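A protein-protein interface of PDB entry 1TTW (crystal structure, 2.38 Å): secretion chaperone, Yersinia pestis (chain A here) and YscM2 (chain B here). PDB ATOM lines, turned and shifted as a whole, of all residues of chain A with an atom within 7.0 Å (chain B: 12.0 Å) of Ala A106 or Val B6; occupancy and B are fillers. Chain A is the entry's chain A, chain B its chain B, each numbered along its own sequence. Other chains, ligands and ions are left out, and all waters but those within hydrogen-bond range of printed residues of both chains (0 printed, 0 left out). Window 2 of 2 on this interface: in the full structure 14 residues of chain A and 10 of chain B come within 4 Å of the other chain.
The backbone carbonyl oxygen of Ala A106 is in hydrogen-bond range of the side-chain hydroxyl of Thr A110 (3.0 Å).
Leu A15 touches Val B6.
CG1 of Val B6 touches CD1 of Ile A32, 3.9 Å away.
Ile A32 touches Thr B8 (CA to CB, 3.8 Å).
Asp A33 touches Ser B7.
Thr B8 touches Asp A33.
Ala A106 touches Val B6 (CB to CG2, 3.5 Å).
Leu A109 touches Val B6.
Val B6 touches Thr A110 (CG1 to OG1, 3.5 Å).
No residue of chain B comes within 4 Å of Phe A11.
Glu A14 touches none of the printed residues of chain B.
Leu A15 touches just one residue of chain B: Val B6.
Printed residues of chain B within 4 Å of Ile A32: Val B6 (3.9 Å) and Thr B8 (3.8 Å).
Of the printed residues of chain B, Asp A33 touches Ser B7 and Thr B8.
Thr A103 touches none of the printed residues of chain B.
Leu A105 touches none of the printed residues of chain B.
Of chain B, only Val B6 comes within 4 Å of Ala A106.
No residue of chain B comes within 4 Å of Ser A107.
No residue of chain B comes within 4 Å of Val A108.
Leu A109 touches just one residue of chain B: Val B6.
Thr A110 touches just one residue of chain B: Val B6.
Of chain A, only Leu A15 (3.6 Å), Ile A32 (3.9 Å), Ala A106 (3.5 Å), Leu A109 (3.9 Å) and Thr A110 (3.5 Å) come within 4 Å of Val B6.
Printed residues of chain A within 4 Å of Ser B7: Asp A33.
Printed residues of chain A within 4 Å of Thr B8: Ile A32 and Asp A33.
The nearest residue of chain B that does not touch Ala A106 is Ser B7 (7.8 Å).
The nearest residue of chain A that does not touch Val B6 is Ser A107 (5.3 Å).
The nearest printed residue of chain B that does not touch Ile A32 is Gln B9 (5.0 Å).
Printed residues of chain B that touch a printed residue of chain A: Val B6, Ser B7 and Thr B8.
Hydrophobic or aromatic side chains of chain B within 4 Å of the printed part of chain A: Val B6.
Of the 20 printed residues of chain A, 6 touch a printed residue of chain B.
Printed residues of chain A that touch a printed residue of chain B: Leu A15, Ile A32, Asp A33, Ala A106, Leu A109 and Thr A110.
Hydrophobic or aromatic side chains of chain A that line the printed part of chain B: Leu A15, Ile A32, Ala A106 and Leu A109.
Along chain A the printed residues that touch a printed residue of chain B span positions 15 to 110.
Among the printed residues, 8 pairs touch across the chains.
Among the printed residues, no Asp or Glu carboxylate lies within 4 Å of a Lys or Arg side-chain nitrogen of the other chain.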
ATOM      1  N   PHE A  11      -4.807  10.241 -16.855  1.00  0.00           N
ATOM      2  CA  PHE A  11      -5.699   9.282 -17.453  1.00  0.00           C
ATOM      3  C   PHE A  11      -6.866  10.146 -17.839  1.00  0.00           C
ATOM      4  O   PHE A  11      -7.367  10.027 -18.944  1.00  0.00           O
ATOM      5  CB  PHE A  11      -6.055   8.215 -16.405  1.00  0.00           C
ATOM      6  CG  PHE A  11      -7.152   7.309 -16.781  1.00  0.00           C
ATOM      7  CD1 PHE A  11      -6.966   6.334 -17.686  1.00  0.00           C
ATOM      8  CD2 PHE A  11      -8.372   7.395 -16.181  1.00  0.00           C
ATOM      9  CE1 PHE A  11      -7.989   5.423 -18.034  1.00  0.00           C
ATOM     10  CE2 PHE A  11      -9.400   6.478 -16.501  1.00  0.00           C
ATOM     11  CZ  PHE A  11      -9.179   5.471 -17.425  1.00  0.00           C
ATOM     12  N   GLU A  14      -5.433  12.295 -21.385  1.00  0.00           N
ATOM     13  CA  GLU A  14      -5.568  11.312 -22.461  1.00  0.00           C
ATOM     14  C   GLU A  14      -7.030  10.776 -22.699  1.00  0.00           C
ATOM     15  O   GLU A  14      -7.259   9.880 -23.542  1.00  0.00           O
ATOM     16  CB  GLU A  14      -4.575  10.102 -22.213  1.00  0.00           C
ATOM     17  N   LEU A  15      -8.004  11.314 -21.964  1.00  0.00           N
ATOM     18  CA  LEU A  15      -9.409  11.008 -22.186  1.00  0.00           C
ATOM     19  C   LEU A  15     -10.409  12.209 -22.071  1.00  0.00           C
ATOM     20  O   LEU A  15     -11.601  11.963 -21.882  1.00  0.00           O
ATOM     21  CB  LEU A  15      -9.787   9.900 -21.178  1.00  0.00           C
ATOM     22  CG  LEU A  15     -10.182   8.537 -21.694  1.00  0.00           C
ATOM     23  CD1 LEU A  15      -9.553   8.200 -23.023  1.00  0.00           C
ATOM     24  CD2 LEU A  15      -9.847   7.460 -20.667  1.00  0.00           C
ATOM     25  N   VAL A  30     -15.371   4.978 -13.330  1.00  0.00           N
ATOM     26  CA  VAL A  30     -15.570   5.597 -14.660  1.00  0.00           C
ATOM     27  C   VAL A  30     -16.680   4.793 -15.246  1.00  0.00           C
ATOM     28  O   VAL A  30     -16.822   3.576 -14.920  1.00  0.00           O
ATOM     29  CB  VAL A  30     -14.291   5.522 -15.439  1.00  0.00           C
ATOM     30  CG1 VAL A  30     -14.558   5.423 -16.850  1.00  0.00           C
ATOM     31  CG2 VAL A  30     -13.463   6.727 -15.227  1.00  0.00           C
ATOM     32  N   ILE A  32     -18.379   3.406 -18.911  1.00  0.00           N
ATOM     33  CA  ILE A  32     -17.869   3.067 -20.263  1.00  0.00           C
ATOM     34  C   ILE A  32     -18.979   2.527 -21.078  1.00  0.00           C
ATOM     35  O   ILE A  32     -19.681   1.668 -20.561  1.00  0.00           O
ATOM     36  CB  ILE A  32     -16.803   1.996 -20.244  1.00  0.00           C
ATOM     37  CG1 ILE A  32     -15.607   2.520 -19.421  1.00  0.00           C
ATOM     38  CG2 ILE A  32     -16.418   1.688 -21.628  1.00  0.00           C
ATOM     39  CD1 ILE A  32     -14.204   1.766 -19.578  1.00  0.00           C
ATOM     40  N   ASP A  33     -19.084   3.000 -22.347  1.00  0.00           N
ATOM     41  CA  ASP A  33     -20.196   2.697 -23.315  1.00  0.00           C
ATOM     42  C   ASP A  33     -21.465   2.675 -22.504  1.00  0.00           C
ATOM     43  O   ASP A  33     -22.298   1.840 -22.683  1.00  0.00           O
ATOM     44  CB  ASP A  33     -20.054   1.368 -24.072  1.00  0.00           C
ATOM     45  CG  ASP A  33     -18.679   1.166 -24.735  1.00  0.00           C
ATOM     46  OD1 ASP A  33     -18.047   2.135 -25.231  1.00  0.00           O
ATOM     47  OD2 ASP A  33     -18.122   0.022 -24.785  1.00  0.00           O
ATOM     48  N   THR A 100       3.144   3.067 -14.915  1.00  0.00           N
ATOM     49  CA  THR A 100       1.878   2.986 -15.693  1.00  0.00           C
ATOM     50  C   THR A 100       1.504   4.424 -16.158  1.00  0.00           C
ATOM     51  O   THR A 100       1.279   5.258 -15.335  1.00  0.00           O
ATOM     52  CB  THR A 100       0.703   2.338 -14.863  1.00  0.00           C
ATOM     53  OG1 THR A 100       0.980   0.960 -14.466  1.00  0.00           O
ATOM     54  CG2 THR A 100      -0.629   2.262 -15.728  1.00  0.00           C
ATOM     55  N   SER A 101       1.456   4.695 -17.488  1.00  0.00           N
ATOM     56  CA  SER A 101       1.178   6.061 -18.006  1.00  0.00           C
ATOM     57  C   SER A 101      -0.314   6.171 -18.042  1.00  0.00           C
ATOM     58  O   SER A 101      -1.037   5.122 -17.984  1.00  0.00           O
ATOM     59  CB  SER A 101       1.694   6.155 -19.431  1.00  0.00           C
ATOM     60  OG  SER A 101       0.985   5.148 -20.182  1.00  0.00           O
ATOM     61  N   GLY A 102      -0.825   7.381 -18.234  1.00  0.00           N
ATOM     62  CA  GLY A 102      -2.288   7.489 -18.344  1.00  0.00           C
ATOM     63  C   GLY A 102      -2.838   6.724 -19.551  1.00  0.00           C
ATOM     64  O   GLY A 102      -3.902   6.113 -19.582  1.00  0.00           O
ATOM     65  N   THR A 103      -2.039   6.675 -20.580  1.00  0.00           N
ATOM     66  CA  THR A 103      -2.467   5.935 -21.744  1.00  0.00           C
ATOM     67  C   THR A 103      -2.320   4.347 -21.598  1.00  0.00           C
ATOM     68  O   THR A 103      -3.050   3.537 -22.215  1.00  0.00           O
ATOM     69  CB  THR A 103      -1.692   6.524 -22.947  1.00  0.00           C
ATOM     70  OG1 THR A 103      -0.803   5.541 -23.373  1.00  0.00           O
ATOM     71  CG2 THR A 103      -0.643   7.616 -22.563  1.00  0.00           C
ATOM     72  N   GLN A 104      -1.405   3.859 -20.738  1.00  0.00           N
ATOM     73  CA  GLN A 104      -1.466   2.409 -20.338  1.00  0.00           C
ATOM     74  C   GLN A 104      -2.708   2.141 -19.568  1.00  0.00           C
ATOM     75  O   GLN A 104      -3.490   1.203 -19.921  1.00  0.00           O
ATOM     76  CB  GLN A 104      -0.165   1.908 -19.795  1.00  0.00           C
ATOM     77  CG  GLN A 104       1.047   2.213 -20.882  1.00  0.00           C
ATOM     78  CD  GLN A 104       2.279   1.240 -20.851  1.00  0.00           C
ATOM     79  OE1 GLN A 104       2.093  -0.036 -20.805  1.00  0.00           O
ATOM     80  NE2 GLN A 104       3.548   1.827 -20.892  1.00  0.00           N
ATOM     81  N   LEU A 105      -3.068   3.029 -18.660  1.00  0.00           N
ATOM     82  CA  LEU A 105      -4.241   2.698 -18.009  1.00  0.00           C
ATOM     83  C   LEU A 105      -5.456   2.558 -18.944  1.00  0.00           C
ATOM     84  O   LEU A 105      -6.329   1.675 -18.836  1.00  0.00           O
ATOM     85  CB  LEU A 105      -4.543   3.811 -17.037  1.00  0.00           C
ATOM     86  CG  LEU A 105      -4.932   3.398 -15.661  1.00  0.00           C
ATOM     87  CD1 LEU A 105      -5.480   4.569 -15.094  1.00  0.00           C
ATOM     88  CD2 LEU A 105      -5.922   2.296 -15.652  1.00  0.00           C
ATOM     89  N   ALA A 106      -5.632   3.519 -19.828  1.00  0.00           N
ATOM     90  CA  ALA A 106      -6.817   3.420 -20.795  1.00  0.00           C
ATOM     91  C   ALA A 106      -6.802   2.193 -21.601  1.00  0.00           C
ATOM     92  O   ALA A 106      -7.734   1.324 -21.778  1.00  0.00           O
ATOM     93  CB  ALA A 106      -6.762   4.664 -21.638  1.00  0.00           C
ATOM     94  N   SER A 107      -5.632   1.885 -21.943  1.00  0.00           N
ATOM     95  CA  SER A 107      -5.425   0.598 -22.546  1.00  0.00           C
ATOM     96  C   SER A 107      -5.929  -0.551 -21.628  1.00  0.00           C
ATOM     97  O   SER A 107      -6.688  -1.498 -22.054  1.00  0.00           O
ATOM     98  CB  SER A 107      -3.956   0.619 -22.874  1.00  0.00           C
ATOM     99  OG  SER A 107      -3.616  -0.438 -23.809  1.00  0.00           O
ATOM    100  N   VAL A 108      -5.705  -0.480 -20.272  1.00  0.00           N
ATOM    101  CA  VAL A 108      -6.091  -1.687 -19.508  1.00  0.00           C
ATOM    102  C   VAL A 108      -7.551  -1.668 -19.519  1.00  0.00           C
ATOM    103  O   VAL A 108      -8.250  -2.676 -19.483  1.00  0.00           O
ATOM    104  CB  VAL A 108      -5.571  -1.591 -18.049  1.00  0.00           C
ATOM    105  CG1 VAL A 108      -6.375  -2.505 -17.105  1.00  0.00           C
ATOM    106  CG2 VAL A 108      -4.075  -1.830 -18.085  1.00  0.00           C
ATOM    107  N   LEU A 109      -8.106  -0.533 -19.431  1.00  0.00           N
ATOM    108  CA  LEU A 109      -9.598  -0.539 -19.304  1.00  0.00           C
ATOM    109  C   LEU A 109     -10.368  -1.071 -20.473  1.00  0.00           C
ATOM    110  O   LEU A 109     -11.492  -1.662 -20.347  1.00  0.00           O
ATOM    111  CB  LEU A 109     -10.121   0.844 -19.186  1.00  0.00           C
ATOM    112  CG  LEU A 109      -9.755   1.764 -18.058  1.00  0.00           C
ATOM    113  CD1 LEU A 109     -10.970   2.671 -17.730  1.00  0.00           C
ATOM    114  CD2 LEU A 109      -8.997   1.097 -16.724  1.00  0.00           C
ATOM    115  N   THR A 110      -9.765  -0.825 -21.638  1.00  0.00           N
ATOM    116  CA  THR A 110     -10.297  -1.302 -22.908  1.00  0.00           C
ATOM    117  C   THR A 110     -10.126  -2.693 -22.813  1.00  0.00           C
ATOM    118  O   THR A 110     -11.050  -3.384 -23.142  1.00  0.00           O
ATOM    119  CB  THR A 110      -9.345  -0.726 -24.113  1.00  0.00           C
ATOM    120  OG1 THR A 110      -9.458   0.700 -24.184  1.00  0.00           O
ATOM    121  CG2 THR A 110      -9.741  -1.217 -25.469  1.00  0.00           C
ATOM    122  N   SER A 111      -8.962  -3.218 -22.474  1.00  0.00           N
ATOM    123  CA  SER A 111      -8.986  -4.659 -22.294  1.00  0.00           C
ATOM    124  C   SER A 111      -9.953  -5.178 -21.255  1.00  0.00           C
ATOM    125  O   SER A 111     -10.561  -6.208 -21.363  1.00  0.00           O
ATOM    126  CB  SER A 111      -7.667  -5.172 -21.906  1.00  0.00           C
ATOM    127  OG  SER A 111      -6.743  -4.625 -22.825  1.00  0.00           O
ATOM    128  N   LEU A 112     -10.240  -4.385 -20.294  1.00  0.00           N
ATOM    129  CA  LEU A 112     -11.065  -4.932 -19.297  1.00  0.00           C
ATOM    130  C   LEU A 112     -12.404  -5.107 -20.047  1.00  0.00           C
ATOM    131  O   LEU A 112     -13.025  -6.126 -19.967  1.00  0.00           O
ATOM    132  CB  LEU A 112     -11.135  -3.997 -18.064  1.00  0.00           C
ATOM    133  CG  LEU A 112     -11.060  -4.227 -16.530  1.00  0.00           C
ATOM    134  CD1 LEU A 112     -10.556  -5.600 -16.082  1.00  0.00           C
ATOM    135  CD2 LEU A 112     -10.262  -3.113 -15.911  1.00  0.00           C
ATOM    136  N   VAL A 113     -12.916  -4.022 -20.567  1.00  0.00           N
ATOM    137  CA  VAL A 113     -14.197  -4.049 -21.275  1.00  0.00           C
ATOM    138  C   VAL A 113     -14.235  -5.006 -22.454  1.00  0.00           C
ATOM    139  O   VAL A 113     -15.145  -5.785 -22.550  1.00  0.00           O
ATOM    140  CB  VAL A 113     -14.568  -2.675 -21.724  1.00  0.00           C
ATOM    141  CG1 VAL A 113     -15.925  -2.726 -22.239  1.00  0.00           C
ATOM    142  CG2 VAL A 113     -14.648  -1.812 -20.575  1.00  0.00           C
ATOM    143  N   VAL B   6     -10.479   3.768 -25.606  1.00  0.00           N
ATOM    144  CA  VAL B   6     -11.683   3.710 -24.698  1.00  0.00           C
ATOM    145  C   VAL B   6     -12.589   4.857 -25.129  1.00  0.00           C
ATOM    146  O   VAL B   6     -12.061   5.982 -25.401  1.00  0.00           O
ATOM    147  CB  VAL B   6     -11.369   3.999 -23.192  1.00  0.00           C
ATOM    148  CG1 VAL B   6     -11.561   2.768 -22.265  1.00  0.00           C
ATOM    149  CG2 VAL B   6     -10.004   4.608 -23.053  1.00  0.00           C
ATOM    150  N   SER B   7     -13.927   4.595 -25.098  1.00  0.00           N
ATOM    151  CA  SER B   7     -14.995   5.401 -25.753  1.00  0.00           C
ATOM    152  C   SER B   7     -15.888   6.392 -24.907  1.00  0.00           C
ATOM    153  O   SER B   7     -16.302   7.413 -25.482  1.00  0.00           O
ATOM    154  CB  SER B   7     -15.907   4.432 -26.595  1.00  0.00           C
ATOM    155  N   THR B   8     -16.156   6.121 -23.598  1.00  0.00           N
ATOM    156  CA  THR B   8     -17.096   6.911 -22.706  1.00  0.00           C
ATOM    157  C   THR B   8     -16.541   7.440 -21.292  1.00  0.00           C
ATOM    158  O   THR B   8     -15.354   7.197 -20.981  1.00  0.00           O
ATOM    159  CB  THR B   8     -18.363   6.098 -22.480  1.00  0.00           C
ATOM    160  N   GLN B   9     -17.410   8.085 -20.449  1.00  0.00           N
ATOM    161  CA  GLN B   9     -16.985   8.988 -19.307  1.00  0.00           C
ATOM    162  C   GLN B   9     -17.715   9.020 -17.843  1.00  0.00           C
ATOM    163  O   GLN B   9     -18.551   8.190 -17.550  1.00  0.00           O
ATOM    164  CB  GLN B   9     -16.817  10.408 -19.864  1.00  0.00           C
ATOM    165  N   ALA B  10     -17.373  10.032 -16.999  1.00  0.00           N
ATOM    166  CA  ALA B  10     -17.320  10.071 -15.477  1.00  0.00           C
ATOM    167  C   ALA B  10     -18.501   9.849 -14.463  1.00  0.00           C
ATOM    168  O   ALA B  10     -19.025  10.844 -14.066  1.00  0.00           O
ATOM    169  CB  ALA B  10     -16.615  11.516 -15.061  1.00  0.00           C
